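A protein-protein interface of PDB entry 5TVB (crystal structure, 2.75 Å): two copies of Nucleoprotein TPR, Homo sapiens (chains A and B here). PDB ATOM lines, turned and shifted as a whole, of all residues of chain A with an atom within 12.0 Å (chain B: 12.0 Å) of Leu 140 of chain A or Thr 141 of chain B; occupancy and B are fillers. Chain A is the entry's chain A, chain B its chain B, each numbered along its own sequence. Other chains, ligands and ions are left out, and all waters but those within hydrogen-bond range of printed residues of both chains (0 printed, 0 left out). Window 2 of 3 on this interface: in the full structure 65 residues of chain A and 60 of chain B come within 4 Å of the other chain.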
ATOM      1  N   GLU A 131      24.099  -9.235 -30.949  1.00  0.00           N
ATOM      2  CA  GLU A 131      24.853 -10.486 -30.907  1.00  0.00           C
ATOM      3  C   GLU A 131      25.413 -10.771 -29.519  1.00  0.00           C
ATOM      4  O   GLU A 131      25.319 -11.893 -29.020  1.00  0.00           O
ATOM      5  CB  GLU A 131      26.004 -10.454 -31.913  1.00  0.00           C
ATOM      6  CG  GLU A 131      25.597 -10.670 -33.357  1.00  0.00           C
ATOM      7  CD  GLU A 131      26.765 -10.505 -34.310  1.00  0.00           C
ATOM      8  OE1 GLU A 131      27.920 -10.683 -33.868  1.00  0.00           O
ATOM      9  OE2 GLU A 131      26.531 -10.197 -35.498  1.00  0.00           O
ATOM     10  N   ARG A 132      25.994  -9.748 -28.903  1.00  0.00           N
ATOM     11  CA  ARG A 132      26.630  -9.897 -27.600  1.00  0.00           C
ATOM     12  C   ARG A 132      25.622 -10.265 -26.521  1.00  0.00           C
ATOM     13  O   ARG A 132      25.881 -11.139 -25.697  1.00  0.00           O
ATOM     14  CB  ARG A 132      27.367  -8.613 -27.217  1.00  0.00           C
ATOM     15  CG  ARG A 132      28.138  -8.710 -25.911  1.00  0.00           C
ATOM     16  CD  ARG A 132      28.939  -7.447 -25.651  1.00  0.00           C
ATOM     17  NE  ARG A 132      28.196  -6.244 -26.014  1.00  0.00           N
ATOM     18  CZ  ARG A 132      27.325  -5.632 -25.220  1.00  0.00           C
ATOM     19  NH1 ARG A 132      27.079  -6.109 -24.008  1.00  0.00           N
ATOM     20  NH2 ARG A 132      26.699  -4.542 -25.640  1.00  0.00           N
ATOM     21  N   LEU A 133      24.474  -9.597 -26.529  1.00  0.00           N
ATOM     22  CA  LEU A 133      23.418  -9.906 -25.575  1.00  0.00           C
ATOM     23  C   LEU A 133      22.877 -11.312 -25.806  1.00  0.00           C
ATOM     24  O   LEU A 133      22.749 -12.096 -24.867  1.00  0.00           O
ATOM     25  CB  LEU A 133      22.282  -8.887 -25.675  1.00  0.00           C
ATOM     26  CG  LEU A 133      22.607  -7.431 -25.339  1.00  0.00           C
ATOM     27  CD1 LEU A 133      21.379  -6.557 -25.542  1.00  0.00           C
ATOM     28  CD2 LEU A 133      23.147  -7.287 -23.925  1.00  0.00           C
ATOM     29  N   SER A 134      22.565 -11.620 -27.062  1.00  0.00           N
ATOM     30  CA  SER A 134      22.058 -12.938 -27.438  1.00  0.00           C
ATOM     31  C   SER A 134      22.999 -14.064 -27.020  1.00  0.00           C
ATOM     32  O   SER A 134      22.576 -15.038 -26.399  1.00  0.00           O
ATOM     33  CB  SER A 134      21.814 -13.005 -28.948  1.00  0.00           C
ATOM     34  OG  SER A 134      20.935 -11.977 -29.369  1.00  0.00           O
ATOM     35  N   GLN A 135      24.274 -13.923 -27.369  1.00  0.00           N
ATOM     36  CA  GLN A 135      25.285 -14.915 -27.016  1.00  0.00           C
ATOM     37  C   GLN A 135      25.432 -15.067 -25.503  1.00  0.00           C
ATOM     38  O   GLN A 135      25.422 -16.182 -24.980  1.00  0.00           O
ATOM     39  CB  GLN A 135      26.635 -14.547 -27.633  1.00  0.00           C
ATOM     40  CG  GLN A 135      27.725 -15.578 -27.390  1.00  0.00           C
ATOM     41  CD  GLN A 135      27.424 -16.909 -28.053  1.00  0.00           C
ATOM     42  OE1 GLN A 135      27.222 -16.980 -29.265  1.00  0.00           O
ATOM     43  NE2 GLN A 135      27.386 -17.971 -27.256  1.00  0.00           N
ATOM     44  N   GLU A 136      25.572 -13.941 -24.811  1.00  0.00           N
ATOM     45  CA  GLU A 136      25.709 -13.936 -23.357  1.00  0.00           C
ATOM     46  C   GLU A 136      24.498 -14.576 -22.689  1.00  0.00           C
ATOM     47  O   GLU A 136      24.617 -15.222 -21.648  1.00  0.00           O
ATOM     48  CB  GLU A 136      25.904 -12.509 -22.847  1.00  0.00           C
ATOM     49  CG  GLU A 136      26.119 -12.408 -21.349  1.00  0.00           C
ATOM     50  CD  GLU A 136      26.403 -10.989 -20.906  1.00  0.00           C
ATOM     51  OE1 GLU A 136      26.658 -10.134 -21.781  1.00  0.00           O
ATOM     52  OE2 GLU A 136      26.371 -10.729 -19.685  1.00  0.00           O
ATOM     53  N   LEU A 137      23.335 -14.390 -23.299  1.00  0.00           N
ATOM     54  CA  LEU A 137      22.101 -14.994 -22.816  1.00  0.00           C
ATOM     55  C   LEU A 137      22.170 -16.519 -22.888  1.00  0.00           C
ATOM     56  O   LEU A 137      21.692 -17.209 -21.989  1.00  0.00           O
ATOM     57  CB  LEU A 137      20.906 -14.472 -23.616  1.00  0.00           C
ATOM     58  CG  LEU A 137      19.510 -14.773 -23.072  1.00  0.00           C
ATOM     59  CD1 LEU A 137      18.607 -13.567 -23.257  1.00  0.00           C
ATOM     60  CD2 LEU A 137      18.915 -15.990 -23.762  1.00  0.00           C
ATOM     61  N   GLU A 138      22.759 -17.036 -23.964  1.00  0.00           N
ATOM     62  CA  GLU A 138      22.887 -18.480 -24.159  1.00  0.00           C
ATOM     63  C   GLU A 138      23.643 -19.166 -23.022  1.00  0.00           C
ATOM     64  O   GLU A 138      23.363 -20.322 -22.699  1.00  0.00           O
ATOM     65  CB  GLU A 138      23.579 -18.787 -25.487  1.00  0.00           C
ATOM     66  CG  GLU A 138      22.652 -18.786 -26.690  1.00  0.00           C
ATOM     67  CD  GLU A 138      23.346 -19.252 -27.954  1.00  0.00           C
ATOM     68  OE1 GLU A 138      24.540 -19.611 -27.879  1.00  0.00           O
ATOM     69  OE2 GLU A 138      22.698 -19.260 -29.024  1.00  0.00           O
ATOM     70  N   TYR A 139      24.602 -18.461 -22.427  1.00  0.00           N
ATOM     71  CA  TYR A 139      25.335 -18.988 -21.278  1.00  0.00           C
ATOM     72  C   TYR A 139      24.393 -19.350 -20.135  1.00  0.00           C
ATOM     73  O   TYR A 139      24.616 -20.321 -19.415  1.00  0.00           O
ATOM     74  CB  TYR A 139      26.369 -17.978 -20.769  1.00  0.00           C
ATOM     75  CG  TYR A 139      27.608 -17.831 -21.621  1.00  0.00           C
ATOM     76  CD1 TYR A 139      28.505 -18.881 -21.770  1.00  0.00           C
ATOM     77  CD2 TYR A 139      27.899 -16.627 -22.251  1.00  0.00           C
ATOM     78  CE1 TYR A 139      29.647 -18.743 -22.540  1.00  0.00           C
ATOM     79  CE2 TYR A 139      29.036 -16.477 -23.021  1.00  0.00           C
ATOM     80  CZ  TYR A 139      29.906 -17.537 -23.162  1.00  0.00           C
ATOM     81  OH  TYR A 139      31.039 -17.391 -23.929  1.00  0.00           O
ATOM     82  N   LEU A 140      23.339 -18.557 -19.976  1.00  0.00           N
ATOM     83  CA  LEU A 140      22.424 -18.712 -18.853  1.00  0.00           C
ATOM     84  C   LEU A 140      21.197 -19.558 -19.190  1.00  0.00           C
ATOM     85  O   LEU A 140      20.300 -19.710 -18.362  1.00  0.00           O
ATOM     86  CB  LEU A 140      21.989 -17.339 -18.337  1.00  0.00           C
ATOM     87  CG  LEU A 140      23.150 -16.398 -18.004  1.00  0.00           C
ATOM     88  CD1 LEU A 140      22.641 -15.006 -17.666  1.00  0.00           C
ATOM     89  CD2 LEU A 140      24.013 -16.961 -16.884  1.00  0.00           C
ATOM     90  N   THR A 141      21.170 -20.127 -20.392  1.00  0.00           N
ATOM     91  CA  THR A 141      20.053 -20.973 -20.798  1.00  0.00           C
ATOM     92  C   THR A 141      20.321 -22.422 -20.415  1.00  0.00           C
ATOM     93  O   THR A 141      21.088 -23.121 -21.077  1.00  0.00           O
ATOM     94  CB  THR A 141      19.802 -20.916 -22.322  1.00  0.00           C
ATOM     95  OG1 THR A 141      20.964 -21.385 -23.020  1.00  0.00           O
ATOM     96  CG2 THR A 141      19.477 -19.500 -22.771  1.00  0.00           C
ATOM     97  N   GLU B 131      16.505  -3.812 -25.893  1.00  0.00           N
ATOM     98  CA  GLU B 131      15.882  -3.548 -24.602  1.00  0.00           C
ATOM     99  C   GLU B 131      15.319  -4.835 -24.023  1.00  0.00           C
ATOM    100  O   GLU B 131      15.469  -5.118 -22.835  1.00  0.00           O
ATOM    101  CB  GLU B 131      14.775  -2.501 -24.735  1.00  0.00           C
ATOM    102  CG  GLU B 131      15.279  -1.072 -24.862  1.00  0.00           C
ATOM    103  CD  GLU B 131      14.160  -0.081 -25.128  1.00  0.00           C
ATOM    104  OE1 GLU B 131      14.446   1.003 -25.680  1.00  0.00           O
ATOM    105  OE2 GLU B 131      12.999  -0.381 -24.778  1.00  0.00           O
ATOM    106  N   ARG B 132      14.673  -5.612 -24.884  1.00  0.00           N
ATOM    107  CA  ARG B 132      14.017  -6.848 -24.485  1.00  0.00           C
ATOM    108  C   ARG B 132      15.022  -7.883 -23.980  1.00  0.00           C
ATOM    109  O   ARG B 132      14.789  -8.536 -22.962  1.00  0.00           O
ATOM    110  CB  ARG B 132      13.213  -7.409 -25.658  1.00  0.00           C
ATOM    111  CG  ARG B 132      12.380  -8.625 -25.317  1.00  0.00           C
ATOM    112  CD  ARG B 132      11.527  -9.051 -26.501  1.00  0.00           C
ATOM    113  NE  ARG B 132      10.541  -8.037 -26.874  1.00  0.00           N
ATOM    114  CZ  ARG B 132       9.306  -7.983 -26.383  1.00  0.00           C
ATOM    115  NH1 ARG B 132       8.906  -8.883 -25.496  1.00  0.00           N
ATOM    116  NH2 ARG B 132       8.472  -7.030 -26.777  1.00  0.00           N
ATOM    117  N   LEU B 133      16.136  -8.033 -24.693  1.00  0.00           N
ATOM    118  CA  LEU B 133      17.210  -8.926 -24.262  1.00  0.00           C
ATOM    119  C   LEU B 133      17.834  -8.446 -22.956  1.00  0.00           C
ATOM    120  O   LEU B 133      18.059  -9.238 -22.041  1.00  0.00           O
ATOM    121  CB  LEU B 133      18.295  -9.047 -25.338  1.00  0.00           C
ATOM    122  CG  LEU B 133      17.960  -9.719 -26.670  1.00  0.00           C
ATOM    123  CD1 LEU B 133      19.156  -9.654 -27.608  1.00  0.00           C
ATOM    124  CD2 LEU B 133      17.550 -11.163 -26.443  1.00  0.00           C
ATOM    125  N   SER B 134      18.116  -7.147 -22.887  1.00  0.00           N
ATOM    126  CA  SER B 134      18.705  -6.534 -21.699  1.00  0.00           C
ATOM    127  C   SER B 134      17.896  -6.856 -20.449  1.00  0.00           C
ATOM    128  O   SER B 134      18.448  -7.278 -19.434  1.00  0.00           O
ATOM    129  CB  SER B 134      18.806  -5.017 -21.877  1.00  0.00           C
ATOM    130  OG  SER B 134      19.518  -4.690 -23.055  1.00  0.00           O
ATOM    131  N   GLN B 135      16.587  -6.655 -20.537  1.00  0.00           N
ATOM    132  CA  GLN B 135      15.680  -6.963 -19.440  1.00  0.00           C
ATOM    133  C   GLN B 135      15.743  -8.446 -19.094  1.00  0.00           C
ATOM    134  O   GLN B 135      15.852  -8.815 -17.925  1.00  0.00           O
ATOM    135  CB  GLN B 135      14.249  -6.561 -19.800  1.00  0.00           C
ATOM    136  CG  GLN B 135      14.061  -5.064 -19.990  1.00  0.00           C
ATOM    137  CD  GLN B 135      12.767  -4.726 -20.703  1.00  0.00           C
ATOM    138  OE1 GLN B 135      11.934  -5.598 -20.952  1.00  0.00           O
ATOM    139  NE2 GLN B 135      12.595  -3.453 -21.042  1.00  0.00           N
ATOM    140  N   GLU B 136      15.671  -9.287 -20.120  1.00  0.00           N
ATOM    141  CA  GLU B 136      15.727 -10.733 -19.943  1.00  0.00           C
ATOM    142  C   GLU B 136      17.014 -11.189 -19.262  1.00  0.00           C
ATOM    143  O   GLU B 136      17.003 -12.136 -18.476  1.00  0.00           O
ATOM    144  CB  GLU B 136      15.581 -11.435 -21.293  1.00  0.00           C
ATOM    145  CG  GLU B 136      14.247 -12.132 -21.484  1.00  0.00           C
ATOM    146  CD  GLU B 136      14.103 -13.353 -20.599  1.00  0.00           C
ATOM    147  OE1 GLU B 136      14.971 -14.248 -20.677  1.00  0.00           O
ATOM    148  OE2 GLU B 136      13.128 -13.417 -19.821  1.00  0.00           O
ATOM    149  N   LEU B 137      18.121 -10.516 -19.563  1.00  0.00           N
ATOM    150  CA  LEU B 137      19.389 -10.824 -18.910  1.00  0.00           C
ATOM    151  C   LEU B 137      19.345 -10.510 -17.420  1.00  0.00           C
ATOM    152  O   LEU B 137      19.774 -11.316 -16.599  1.00  0.00           O
ATOM    153  CB  LEU B 137      20.537 -10.048 -19.562  1.00  0.00           C
ATOM    154  CG  LEU B 137      21.145 -10.632 -20.836  1.00  0.00           C
ATOM    155  CD1 LEU B 137      22.268  -9.742 -21.339  1.00  0.00           C
ATOM    156  CD2 LEU B 137      21.650 -12.044 -20.589  1.00  0.00           C
ATOM    157  N   GLU B 138      18.812  -9.341 -17.078  1.00  0.00           N
ATOM    158  CA  GLU B 138      18.722  -8.918 -15.684  1.00  0.00           C
ATOM    159  C   GLU B 138      17.857  -9.870 -14.867  1.00  0.00           C
ATOM    160  O   GLU B 138      18.123 -10.109 -13.691  1.00  0.00           O
ATOM    161  CB  GLU B 138      18.175  -7.493 -15.594  1.00  0.00           C
ATOM    162  CG  GLU B 138      18.292  -6.879 -14.212  1.00  0.00           C
ATOM    163  CD  GLU B 138      18.356  -5.365 -14.255  1.00  0.00           C
ATOM    164  OE1 GLU B 138      18.300  -4.798 -15.367  1.00  0.00           O
ATOM    165  OE2 GLU B 138      18.467  -4.743 -13.177  1.00  0.00           O
ATOM    166  N   TYR B 139      16.818 -10.402 -15.502  1.00  0.00           N
ATOM    167  CA  TYR B 139      15.952 -11.394 -14.879  1.00  0.00           C
ATOM    168  C   TYR B 139      16.711 -12.662 -14.488  1.00  0.00           C
ATOM    169  O   TYR B 139      16.423 -13.276 -13.462  1.00  0.00           O
ATOM    170  CB  TYR B 139      14.793 -11.748 -15.815  1.00  0.00           C
ATOM    171  CG  TYR B 139      13.915 -12.869 -15.306  1.00  0.00           C
ATOM    172  CD1 TYR B 139      13.072 -12.677 -14.221  1.00  0.00           C
ATOM    173  CD2 TYR B 139      13.927 -14.117 -15.915  1.00  0.00           C
ATOM    174  CE1 TYR B 139      12.267 -13.700 -13.752  1.00  0.00           C
ATOM    175  CE2 TYR B 139      13.126 -15.145 -15.455  1.00  0.00           C
ATOM    176  CZ  TYR B 139      12.299 -14.932 -14.372  1.00  0.00           C
ATOM    177  OH  TYR B 139      11.497 -15.952 -13.912  1.00  0.00           O
ATOM    178  N   LEU B 140      17.663 -13.061 -15.328  1.00  0.00           N
ATOM    179  CA  LEU B 140      18.396 -14.308 -15.125  1.00  0.00           C
ATOM    180  C   LEU B 140      19.754 -14.152 -14.446  1.00  0.00           C
ATOM    181  O   LEU B 140      20.478 -15.130 -14.274  1.00  0.00           O
ATOM    182  CB  LEU B 140      18.600 -15.006 -16.470  1.00  0.00           C
ATOM    183  CG  LEU B 140      17.361 -15.295 -17.313  1.00  0.00           C
ATOM    184  CD1 LEU B 140      17.787 -15.705 -18.706  1.00  0.00           C
ATOM    185  CD2 LEU B 140      16.545 -16.402 -16.673  1.00  0.00           C
ATOM    186  N   THR B 141      20.121 -12.926 -14.100  1.00  0.00           N
ATOM    187  CA  THR B 141      21.381 -12.693 -13.404  1.00  0.00           C
ATOM    188  C   THR B 141      21.164 -12.321 -11.939  1.00  0.00           C
ATOM    189  O   THR B 141      20.695 -13.134 -11.143  1.00  0.00           O
ATOM    190  CB  THR B 141      22.209 -11.608 -14.108  1.00  0.00           C
ATOM    191  OG1 THR B 141      21.455 -10.392 -14.164  1.00  0.00           O
ATOM    192  CG2 THR B 141      22.551 -12.052 -15.524  1.00  0.00           C
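The backbone carbonyl oxygen of Leu 137 of chain B sits close to the side-chain hydroxyl of Thr 141 of chain B (3.1 Å).
The backbone carbonyl oxygen (O) of Glu 138 of chain B lies within hydrogen-bond range of the side-chain hydroxyl (OG1) of Thr 141 of chain B (3.4 Å).
Leu 133 of chain A touches Leu 133 of chain B (CB to CD1, 3.8 Å).
Ser 134 of chain B touches Leu 133 of chain A (OG to CD1, 3.6 Å).
Leu 137 of chain B touches Leu 133 of chain A (CD1 to CD2, 3.7 Å).
Ser 134 of chain A touches Leu 133 of chain B (OG to CD1, 3.4 Å).
CA of Leu 137 of chain A touches CD2 of Leu 137 of chain B, at 3.7 Å.
CD1 of Leu 140 of chain A touches CG2 of Thr 141 of chain B (3.6 Å).
Printed residues of chain B within 4 Å of Leu 133 of chain A: Leu 133 (3.8 Å), Ser 134 (3.6 Å) and Leu 137 (3.7 Å).
Of the printed residues of chain B, Ser 134 of chain A touches Leu 133.
Glu 136 of chain A touches none of the printed residues of chain B.
Of chain B, only Leu 137 comes within 4 Å of Leu 137 of chain A.
Leu 140 of chain A touches just one residue of chain B: Thr 141.
Printed residues of chain A within 4 Å of Leu 133 of chain B: Leu 133 and Ser 134.
Of the printed residues of chain A, Ser 134 of chain B touches Leu 133.
Leu 137 of chain B touches just these residues of chain A: Leu 133 and Leu 137.
No residue of chain A comes within 4 Å of Glu 138 of chain B.
No residue of chain A comes within 4 Å of Leu 140 of chain B.
Thr 141 of chain B touches one residue of chain A.
Printed residues of chain A that touch a printed residue of chain B: Leu 133, Ser 134, Leu 137 and Leu 140.
Hydrophobic or aromatic side chains of chain A within 4 Å of the printed part of chain B: Leu 133, Leu 137 and Leu 140.
Of the 11 printed residues of chain B, 4 touch a printed residue of chain A.
Hydrophobic or aromatic side chains of chain B that line the printed part of chain A: Leu 133 and Leu 137.
Among the printed residues, 6 pairs touch across the chains.
Among the printed residues, no Asp or Glu carboxylate lies within 4 Å of a Lys or Arg side-chain nitrogen of the other chain.
Leu 133 of chain B touches its own counterpart, Leu 133 of chain A.
Leu 133 of chain A touches Ser 134 of chain B, and with the chains exchanged Ser 134 of chain A touches Leu 133 of chain B.
Leu 133 of chain A touches Leu 137 of chain B, but with the chains exchanged Leu 137 of chain A does not touch Leu 133 of chain B (4.1 Å).
Leu 137 of chain A touches its own counterpart, Leu 137 of chain B.
11 positions are printed for both chains.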
